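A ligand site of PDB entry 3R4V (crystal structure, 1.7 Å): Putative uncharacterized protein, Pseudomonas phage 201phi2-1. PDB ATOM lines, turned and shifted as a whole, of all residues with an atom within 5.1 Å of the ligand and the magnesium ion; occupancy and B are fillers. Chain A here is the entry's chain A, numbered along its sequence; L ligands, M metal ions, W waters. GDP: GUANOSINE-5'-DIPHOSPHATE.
An oxygen (O3B) of the ligand sits at hydrogen-bond distance from the backbone NH (N) of Ser 94.
OG of Ser 89 sits at hydrogen-bond distance from O4' of the ligand, at 3.1 Å.
An oxygen (O2A) of the ligand is in hydrogen-bond range of the side-chain hydroxyl (OG1) of Thr 13, at 2.7 Å.
N of Gly 95 is in hydrogen-bond range of O2B of the ligand (2.7 Å).
O3B of the ligand is in hydrogen-bond range of N of Gly 93 (2.8 Å).
The side-chain amide nitrogen (ND2) of Asn 16 is in hydrogen-bond range of an oxygen (O6) of the ligand (2.8 Å).
A nitrogen (N1) of the ligand is in hydrogen-bond range of the side-chain amide oxygen of Asn 165.
O2A of the ligand lies within hydrogen-bond range of N of Thr 13.
The side-chain amide oxygen (OD1) of Asn 155 lies within hydrogen-bond range of a nitrogen (N2) of the ligand, at 2.9 Å.
The side-chain hydroxyl (OH) of Tyr 161 lies within hydrogen-bond range of an oxygen (O2') of the ligand, at 3.2 Å.
An oxygen (O2') of the ligand lies close to the side-chain carboxylate of Glu 122, at 3.4 Å.
The side-chain amide oxygen (OD1) of Asn 126 is in hydrogen-bond range of an oxygen (O2') of the ligand.
The backbone NH (N) of Gly 12 lies close to an oxygen (O1B) of the ligand.
N of Glu 122 is in hydrogen-bond range of OD1 of Asn 126 (3.1 Å).
The backbone carbonyl oxygen (O) of Gly 12 lies close to the side-chain amide oxygen (OD1) of Asn 16, at 3.3 Å.
The backbone carbonyl oxygen of Gly 12 is in hydrogen-bond range of the side-chain amide nitrogen of Asn 37 (3.4 Å).
The side-chain amide oxygen of Asn 16 is in hydrogen-bond range of the side-chain amide nitrogen of Asn 37 (2.9 Å).
The backbone carbonyl oxygen of Gly 91 is in hydrogen-bond range of the side-chain amide nitrogen of Asn 126 (3.1 Å).
OG of Ser 89 sits close to N of Gly 91 (3.2 Å).
O of Tyr 161 lies close to OD1 of Asn 165 (3.2 Å).
OH of Tyr 161 is in hydrogen-bond range of OE2 of Glu 122.
Merely in contact with the ligand: Ile 164 (3.4 Å), Gly 11 (3.4 Å), Ala 120 (3.5 Å), Gly 92 (3.5 Å) and Val 118 (3.7 Å).
Hydrophobic or aromatic side chains within 4 Å of the ligand: Val 118, Ala 120, Tyr 161 and Ile 164.
Of the 25 residues printed, 17 come within 4 Å of the ligand.
The nearest printed residue that does not touch the ligand is Gly 91 (4.1 Å).
No residue comes within 4 Å of the magnesium ion.
The nearest printed residue that does not touch the magnesium ion is Gly 12 (4.01 Å).
Water W10 binds the magnesium ion (2.2 Å).
The magnesium ion is bound by an oxygen (O1B) of the ligand (2.2 Å).
Water W8 is bound to the magnesium ion, at 2.2 Å.
The magnesium ion is bound by water W4, 2.3 Å away.
Water W7 binds the magnesium ion, 2.3 Å away.
Water W11 binds the magnesium ion, 2.3 Å away.
Water W4 lies within hydrogen-bond range of the side-chain carboxylate (OD1) of Asp 32 (2.6 Å), the side-chain amide oxygen (OD1) of Asn 37 (2.6 Å) and the backbone NH (N) of Gly 12 (3.1 Å).
Water W1 lies within hydrogen-bond range of O4' of the ligand (2.5 Å), OG of Ser 89 (2.6 Å) and OG1 of Thr 13 (3.1 Å).
Water W9 bridges O3' of the ligand (2.6 Å) and OE1 of Glu 122 (3.4 Å).
Water W12 lies within hydrogen-bond range of O1A of the ligand (2.7 Å), ND2 of Asn 37 (3.2 Å) and ND2 of Asn 16 (3.4 Å).
Water W2 lies within hydrogen-bond range of the side-chain hydroxyl of Tyr 161 (2.8 Å), an oxygen (O2') of the ligand (2.9 Å), the side-chain amide nitrogen of Asn 155 (2.9 Å) and the backbone NH of Met 121 (3.0 Å).
Water W3 lies within hydrogen-bond range of O of Ala 10, N of Ser 89 and O2A of the ligand.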
ATOM      1  N   ALA A  10     -13.679 -18.815 -16.007  1.00  0.00           N
ATOM      2  CA  ALA A  10     -12.347 -19.190 -15.522  1.00  0.00           C
ATOM      3  C   ALA A  10     -12.096 -18.706 -14.117  1.00  0.00           C
ATOM      4  O   ALA A  10     -12.506 -17.600 -13.741  1.00  0.00           O
ATOM      5  CB  ALA A  10     -11.282 -18.640 -16.455  1.00  0.00           C
ATOM      6  N   GLY A  11     -11.423 -19.544 -13.318  1.00  0.00           N
ATOM      7  CA  GLY A  11     -11.049 -19.185 -11.968  1.00  0.00           C
ATOM      8  C   GLY A  11     -12.252 -19.302 -11.047  1.00  0.00           C
ATOM      9  O   GLY A  11     -13.369 -19.597 -11.493  1.00  0.00           O
ATOM     10  N   GLY A  12     -12.038 -19.071  -9.752  1.00  0.00           N
ATOM     11  CA  GLY A  12     -13.114 -19.131  -8.780  1.00  0.00           C
ATOM     12  C   GLY A  12     -14.318 -18.246  -9.079  1.00  0.00           C
ATOM     13  O   GLY A  12     -15.468 -18.699  -9.022  1.00  0.00           O
ATOM     14  N   THR A  13     -14.059 -16.986  -9.430  1.00  0.00           N
ATOM     15  CA  THR A  13     -15.133 -16.053  -9.681  1.00  0.00           C
ATOM     16  C   THR A  13     -15.972 -16.511 -10.863  1.00  0.00           C
ATOM     17  O   THR A  13     -17.208 -16.479 -10.805  1.00  0.00           O
ATOM     18  CB  THR A  13     -14.608 -14.635  -9.924  1.00  0.00           C
ATOM     19  OG1 THR A  13     -14.039 -14.131  -8.714  1.00  0.00           O
ATOM     20  CG2 THR A  13     -15.740 -13.723 -10.353  1.00  0.00           C
ATOM     21  N   GLY A  14     -15.297 -16.972 -11.918  1.00  0.00           N
ATOM     22  CA  GLY A  14     -15.969 -17.540 -13.069  1.00  0.00           C
ATOM     23  C   GLY A  14     -16.814 -18.749 -12.710  1.00  0.00           C
ATOM     24  O   GLY A  14     -17.934 -18.889 -13.174  1.00  0.00           O
ATOM     25  N   ASN A  16     -18.108 -19.364  -9.818  1.00  0.00           N
ATOM     26  CA  ASN A  16     -19.204 -18.884  -9.001  1.00  0.00           C
ATOM     27  C   ASN A  16     -20.306 -18.276  -9.873  1.00  0.00           C
ATOM     28  O   ASN A  16     -21.486 -18.528  -9.661  1.00  0.00           O
ATOM     29  CB  ASN A  16     -18.729 -17.889  -7.951  1.00  0.00           C
ATOM     30  CG  ASN A  16     -17.801 -18.507  -6.905  1.00  0.00           C
ATOM     31  OD1 ASN A  16     -17.671 -19.738  -6.795  1.00  0.00           O
ATOM     32  ND2 ASN A  16     -17.177 -17.658  -6.099  1.00  0.00           N
ATOM     33  N   ASP A  32     -10.546 -24.173 -14.344  1.00  0.00           N
ATOM     34  CA  ASP A  32      -9.858 -23.736 -13.141  1.00  0.00           C
ATOM     35  C   ASP A  32      -8.630 -24.617 -12.938  1.00  0.00           C
ATOM     36  O   ASP A  32      -8.402 -25.578 -13.671  1.00  0.00           O
ATOM     37  CB  ASP A  32     -10.778 -23.821 -11.906  1.00  0.00           C
ATOM     38  CG  ASP A  32     -10.459 -22.756 -10.857  1.00  0.00           C
ATOM     39  OD1 ASP A  32     -11.306 -22.545  -9.956  1.00  0.00           O
ATOM     40  OD2 ASP A  32      -9.383 -22.124 -10.921  1.00  0.00           O
ATOM     41  N   ASN A  37     -13.801 -24.420  -6.064  1.00  0.00           N
ATOM     42  CA  ASN A  37     -15.060 -23.748  -6.379  1.00  0.00           C
ATOM     43  C   ASN A  37     -16.069 -24.610  -7.094  1.00  0.00           C
ATOM     44  O   ASN A  37     -17.139 -24.131  -7.470  1.00  0.00           O
ATOM     45  CB  ASN A  37     -14.783 -22.492  -7.209  1.00  0.00           C
ATOM     46  CG  ASN A  37     -14.163 -21.390  -6.388  1.00  0.00           C
ATOM     47  OD1 ASN A  37     -12.978 -21.463  -6.052  1.00  0.00           O
ATOM     48  ND2 ASN A  37     -14.943 -20.360  -6.084  1.00  0.00           N
ATOM     49  N   GLY A  58      -3.146 -17.698  -6.609  1.00  0.00           N
ATOM     50  CA  GLY A  58      -3.181 -16.256  -6.433  1.00  0.00           C
ATOM     51  C   GLY A  58      -2.027 -15.523  -7.096  1.00  0.00           C
ATOM     52  O   GLY A  58      -2.099 -14.307  -7.319  1.00  0.00           O
ATOM     53  N   SER A  89     -12.369 -13.185 -12.871  1.00  0.00           N
ATOM     54  CA  SER A  89     -11.841 -12.088 -12.070  1.00  0.00           C
ATOM     55  C   SER A  89     -10.470 -11.624 -12.571  1.00  0.00           C
ATOM     56  O   SER A  89      -9.618 -12.443 -12.911  1.00  0.00           O
ATOM     57  CB  SER A  89     -11.732 -12.489 -10.593  1.00  0.00           C
ATOM     58  OG  SER A  89     -11.292 -11.392  -9.791  1.00  0.00           O
ATOM     59  N   GLY A  91      -8.450 -10.181 -10.625  1.00  0.00           N
ATOM     60  CA  GLY A  91      -7.612 -10.014  -9.443  1.00  0.00           C
ATOM     61  C   GLY A  91      -7.023 -11.248  -8.778  1.00  0.00           C
ATOM     62  O   GLY A  91      -6.229 -11.118  -7.850  1.00  0.00           O
ATOM     63  N   GLY A  92      -7.397 -12.427  -9.240  1.00  0.00           N
ATOM     64  CA  GLY A  92      -6.844 -13.664  -8.693  1.00  0.00           C
ATOM     65  C   GLY A  92      -5.677 -14.150  -9.539  1.00  0.00           C
ATOM     66  O   GLY A  92      -5.111 -13.380 -10.317  1.00  0.00           O
ATOM     67  N   GLY A  93      -5.333 -15.428  -9.391  1.00  0.00           N
ATOM     68  CA  GLY A  93      -4.171 -15.988 -10.044  1.00  0.00           C
ATOM     69  C   GLY A  93      -4.512 -16.901 -11.215  1.00  0.00           C
ATOM     70  O   GLY A  93      -3.728 -17.020 -12.147  1.00  0.00           O
ATOM     71  N   SER A  94      -5.689 -17.534 -11.155  1.00  0.00           N
ATOM     72  CA  SER A  94      -6.054 -18.557 -12.133  1.00  0.00           C
ATOM     73  C   SER A  94      -6.965 -18.054 -13.246  1.00  0.00           C
ATOM     74  O   SER A  94      -6.665 -18.240 -14.433  1.00  0.00           O
ATOM     75  CB  SER A  94      -6.695 -19.771 -11.438  1.00  0.00           C
ATOM     76  OG  SER A  94      -5.775 -20.406 -10.579  1.00  0.00           O
ATOM     77  N   GLY A  95      -8.078 -17.430 -12.860  1.00  0.00           N
ATOM     78  CA  GLY A  95      -8.985 -16.841 -13.834  1.00  0.00           C
ATOM     79  C   GLY A  95      -8.286 -15.796 -14.667  1.00  0.00           C
ATOM     80  O   GLY A  95      -8.486 -15.744 -15.893  1.00  0.00           O
ATOM     81  N   SER A  96      -7.441 -14.987 -14.043  1.00  0.00           N
ATOM     82  CA  SER A  96      -6.809 -13.866 -14.724  1.00  0.00           C
ATOM     83  C   SER A  96      -5.650 -14.315 -15.624  1.00  0.00           C
ATOM     84  O   SER A  96      -5.005 -13.477 -16.253  1.00  0.00           O
ATOM     85  CB  SER A  96      -6.305 -12.839 -13.721  1.00  0.00           C
ATOM     86  OG  SER A  96      -5.215 -13.398 -12.976  1.00  0.00           O
ATOM     87  N   VAL A 118     -14.087  -8.927 -13.434  1.00  0.00           N
ATOM     88  CA  VAL A 118     -14.335  -8.326 -12.128  1.00  0.00           C
ATOM     89  C   VAL A 118     -13.084  -7.620 -11.619  1.00  0.00           C
ATOM     90  O   VAL A 118     -11.998  -8.193 -11.610  1.00  0.00           O
ATOM     91  CB  VAL A 118     -14.792  -9.394 -11.109  1.00  0.00           C
ATOM     92  CG1 VAL A 118     -14.782  -8.841  -9.695  1.00  0.00           C
ATOM     93  CG2 VAL A 118     -16.171  -9.901 -11.458  1.00  0.00           C
ATOM     94  N   ALA A 120     -11.217  -6.808  -8.617  1.00  0.00           N
ATOM     95  CA  ALA A 120     -11.143  -7.246  -7.222  1.00  0.00           C
ATOM     96  C   ALA A 120     -10.402  -6.203  -6.395  1.00  0.00           C
ATOM     97  O   ALA A 120      -9.406  -5.635  -6.860  1.00  0.00           O
ATOM     98  CB  ALA A 120     -10.421  -8.596  -7.138  1.00  0.00           C
ATOM     99  N   MET A 121     -10.844  -5.978  -5.166  1.00  0.00           N
ATOM    100  CA  MET A 121     -10.398  -4.786  -4.454  1.00  0.00           C
ATOM    101  C   MET A 121      -9.899  -5.056  -3.032  1.00  0.00           C
ATOM    102  O   MET A 121      -9.617  -4.112  -2.303  1.00  0.00           O
ATOM    103  CB  MET A 121     -11.531  -3.751  -4.396  1.00  0.00           C
ATOM    104  CG  MET A 121     -12.122  -3.358  -5.733  1.00  0.00           C
ATOM    105  SD  MET A 121     -10.960  -2.472  -6.770  1.00  0.00           S
ATOM    106  CE  MET A 121     -11.984  -2.120  -8.201  1.00  0.00           C
ATOM    107  N   GLU A 122      -9.793  -6.325  -2.648  1.00  0.00           N
ATOM    108  CA  GLU A 122      -9.477  -6.671  -1.260  1.00  0.00           C
ATOM    109  C   GLU A 122      -8.108  -6.193  -0.760  1.00  0.00           C
ATOM    110  O   GLU A 122      -7.963  -5.760   0.389  1.00  0.00           O
ATOM    111  CB  GLU A 122      -9.550  -8.187  -1.049  1.00  0.00           C
ATOM    112  CG  GLU A 122     -10.907  -8.829  -1.229  1.00  0.00           C
ATOM    113  CD  GLU A 122     -10.876 -10.315  -0.898  1.00  0.00           C
ATOM    114  OE1 GLU A 122      -9.780 -10.832  -0.584  1.00  0.00           O
ATOM    115  OE2 GLU A 122     -11.947 -10.972  -0.951  1.00  0.00           O
ATOM    116  N   ASN A 126      -4.642  -8.172  -5.100  1.00  0.00           N
ATOM    117  CA  ASN A 126      -5.783  -8.076  -6.018  1.00  0.00           C
ATOM    118  C   ASN A 126      -5.576  -6.902  -6.983  1.00  0.00           C
ATOM    119  O   ASN A 126      -5.765  -7.026  -8.187  1.00  0.00           O
ATOM    120  CB  ASN A 126      -7.074  -7.803  -5.238  1.00  0.00           C
ATOM    121  CG  ASN A 126      -7.754  -9.057  -4.712  1.00  0.00           C
ATOM    122  OD1 ASN A 126      -8.752  -8.962  -3.998  1.00  0.00           O
ATOM    123  ND2 ASN A 126      -7.236 -10.224  -5.056  1.00  0.00           N
ATOM    124  N   ASN A 155     -15.665  -4.689  -7.679  1.00  0.00           N
ATOM    125  CA  ASN A 155     -16.198  -5.086  -6.391  1.00  0.00           C
ATOM    126  C   ASN A 155     -16.199  -3.890  -5.451  1.00  0.00           C
ATOM    127  O   ASN A 155     -15.262  -3.660  -4.698  1.00  0.00           O
ATOM    128  CB  ASN A 155     -15.363  -6.214  -5.774  1.00  0.00           C
ATOM    129  CG  ASN A 155     -15.566  -7.551  -6.459  1.00  0.00           C
ATOM    130  OD1 ASN A 155     -16.528  -7.743  -7.182  1.00  0.00           O
ATOM    131  ND2 ASN A 155     -14.656  -8.489  -6.212  1.00  0.00           N
ATOM    132  N   TYR A 161     -20.361 -10.359  -2.843  1.00  0.00           N
ATOM    133  CA  TYR A 161     -19.970 -11.008  -4.094  1.00  0.00           C
ATOM    134  C   TYR A 161     -21.193 -11.672  -4.714  1.00  0.00           C
ATOM    135  O   TYR A 161     -21.303 -11.783  -5.935  1.00  0.00           O
ATOM    136  CB  TYR A 161     -18.863 -12.033  -3.834  1.00  0.00           C
ATOM    137  CG  TYR A 161     -17.537 -11.416  -3.428  1.00  0.00           C
ATOM    138  CD1 TYR A 161     -17.322 -10.045  -3.518  1.00  0.00           C
ATOM    139  CD2 TYR A 161     -16.501 -12.210  -2.934  1.00  0.00           C
ATOM    140  CE1 TYR A 161     -16.111  -9.478  -3.146  1.00  0.00           C
ATOM    141  CE2 TYR A 161     -15.295 -11.647  -2.550  1.00  0.00           C
ATOM    142  CZ  TYR A 161     -15.106 -10.278  -2.652  1.00  0.00           C
ATOM    143  OH  TYR A 161     -13.898  -9.725  -2.271  1.00  0.00           O
ATOM    144  N   ILE A 164     -22.937  -8.961  -6.724  1.00  0.00           N
ATOM    145  CA  ILE A 164     -22.192  -8.658  -7.930  1.00  0.00           C
ATOM    146  C   ILE A 164     -22.334  -9.790  -8.942  1.00  0.00           C
ATOM    147  O   ILE A 164     -22.538  -9.542 -10.144  1.00  0.00           O
ATOM    148  CB  ILE A 164     -20.700  -8.377  -7.599  1.00  0.00           C
ATOM    149  CG1 ILE A 164     -20.605  -7.062  -6.823  1.00  0.00           C
ATOM    150  CG2 ILE A 164     -19.854  -8.307  -8.874  1.00  0.00           C
ATOM    151  CD1 ILE A 164     -19.543  -7.067  -5.744  1.00  0.00           C
ATOM    152  N   ASN A 165     -22.253 -11.031  -8.466  1.00  0.00           N
ATOM    153  CA  ASN A 165     -22.369 -12.187  -9.351  1.00  0.00           C
ATOM    154  C   ASN A 165     -23.745 -12.238 -10.014  1.00  0.00           C
ATOM    155  O   ASN A 165     -23.858 -12.567 -11.196  1.00  0.00           O
ATOM    156  CB  ASN A 165     -22.109 -13.498  -8.587  1.00  0.00           C
ATOM    157  CG  ASN A 165     -20.649 -13.684  -8.229  1.00  0.00           C
ATOM    158  OD1 ASN A 165     -19.790 -12.871  -8.585  1.00  0.00           O
ATOM    159  ND2 ASN A 165     -20.359 -14.768  -7.513  1.00  0.00           N
HETATM  160  PB  GDP L   1      -8.798 -17.258  -9.004  1.00  0.00           P
HETATM  161  O1B GDP L   1      -9.480 -18.589  -8.746  1.00  0.00           O
HETATM  162  O2B GDP L   1      -9.079 -16.851 -10.425  1.00  0.00           O
HETATM  163  O3B GDP L   1      -7.304 -17.373  -8.742  1.00  0.00           O
HETATM  164  O3A GDP L   1      -9.352 -16.168  -7.974  1.00  0.00           O
HETATM  165  PA  GDP L   1     -10.892 -15.873  -7.619  1.00  0.00           P
HETATM  166  O1A GDP L   1     -11.547 -17.014  -6.857  1.00  0.00           O
HETATM  167  O2A GDP L   1     -11.672 -15.513  -8.857  1.00  0.00           O
HETATM  168  O5' GDP L   1     -10.710 -14.641  -6.654  1.00  0.00           O
HETATM  169  C5' GDP L   1     -10.009 -13.448  -7.071  1.00  0.00           C
HETATM  170  C4' GDP L   1     -10.519 -12.242  -6.305  1.00  0.00           C
HETATM  171  O4' GDP L   1     -11.846 -11.918  -6.759  1.00  0.00           O
HETATM  172  C3' GDP L   1     -10.667 -12.484  -4.812  1.00  0.00           C
HETATM  173  O3' GDP L   1      -9.479 -12.085  -4.129  1.00  0.00           O
HETATM  174  C2' GDP L   1     -11.826 -11.592  -4.425  1.00  0.00           C
HETATM  175  O2' GDP L   1     -11.383 -10.254  -4.239  1.00  0.00           O
HETATM  176  C1' GDP L   1     -12.710 -11.571  -5.657  1.00  0.00           C
HETATM  177  N9  GDP L   1     -13.739 -12.625  -5.651  1.00  0.00           N
HETATM  178  C8  GDP L   1     -13.624 -13.908  -5.219  1.00  0.00           C
HETATM  179  N7  GDP L   1     -14.777 -14.591  -5.422  1.00  0.00           N
HETATM  180  C5  GDP L   1     -15.651 -13.757  -6.024  1.00  0.00           C
HETATM  181  C6  GDP L   1     -17.039 -13.828  -6.534  1.00  0.00           C
HETATM  182  O6  GDP L   1     -17.688 -14.892  -6.447  1.00  0.00           O
HETATM  183  N1  GDP L   1     -17.571 -12.724  -7.086  1.00  0.00           N
HETATM  184  C2  GDP L   1     -16.872 -11.566  -7.192  1.00  0.00           C
HETATM  185  N2  GDP L   1     -17.452 -10.476  -7.773  1.00  0.00           N
HETATM  186  N3  GDP L   1     -15.603 -11.436  -6.755  1.00  0.00           N
HETATM  187  C4  GDP L   1     -14.954 -12.477  -6.179  1.00  0.00           C
HETATM  188 MG    MG M   1      -9.101 -20.161  -7.244  1.00  0.00          MG
HETATM  189  O   HOH W   1     -13.500 -11.091  -8.464  1.00  0.00           O
HETATM  190  O   HOH W   2     -12.908  -7.821  -3.997  1.00  0.00           O
HETATM  191  O   HOH W   3     -11.698 -15.757 -11.795  1.00  0.00           O
HETATM  192  O   HOH W   4     -11.026 -21.236  -7.773  1.00  0.00           O
HETATM  193  O   HOH W   5      -8.413 -14.355 -11.278  1.00  0.00           O
HETATM  194  O   HOH W   6      -4.799 -19.140  -8.149  1.00  0.00           O
HETATM  195  O   HOH W   7     -10.177 -18.940  -5.664  1.00  0.00           O
HETATM  196  O   HOH W   8      -7.165 -19.166  -6.693  1.00  0.00           O
HETATM  197  O   HOH W   9      -9.565 -13.791  -2.214  1.00  0.00           O
HETATM  198  O   HOH W  10      -8.179 -21.467  -8.739  1.00  0.00           O
HETATM  199  O   HOH W  11      -8.539 -21.859  -5.818  1.00  0.00           O
HETATM  200  O   HOH W  12     -13.800 -17.442  -5.437  1.00  0.00           O
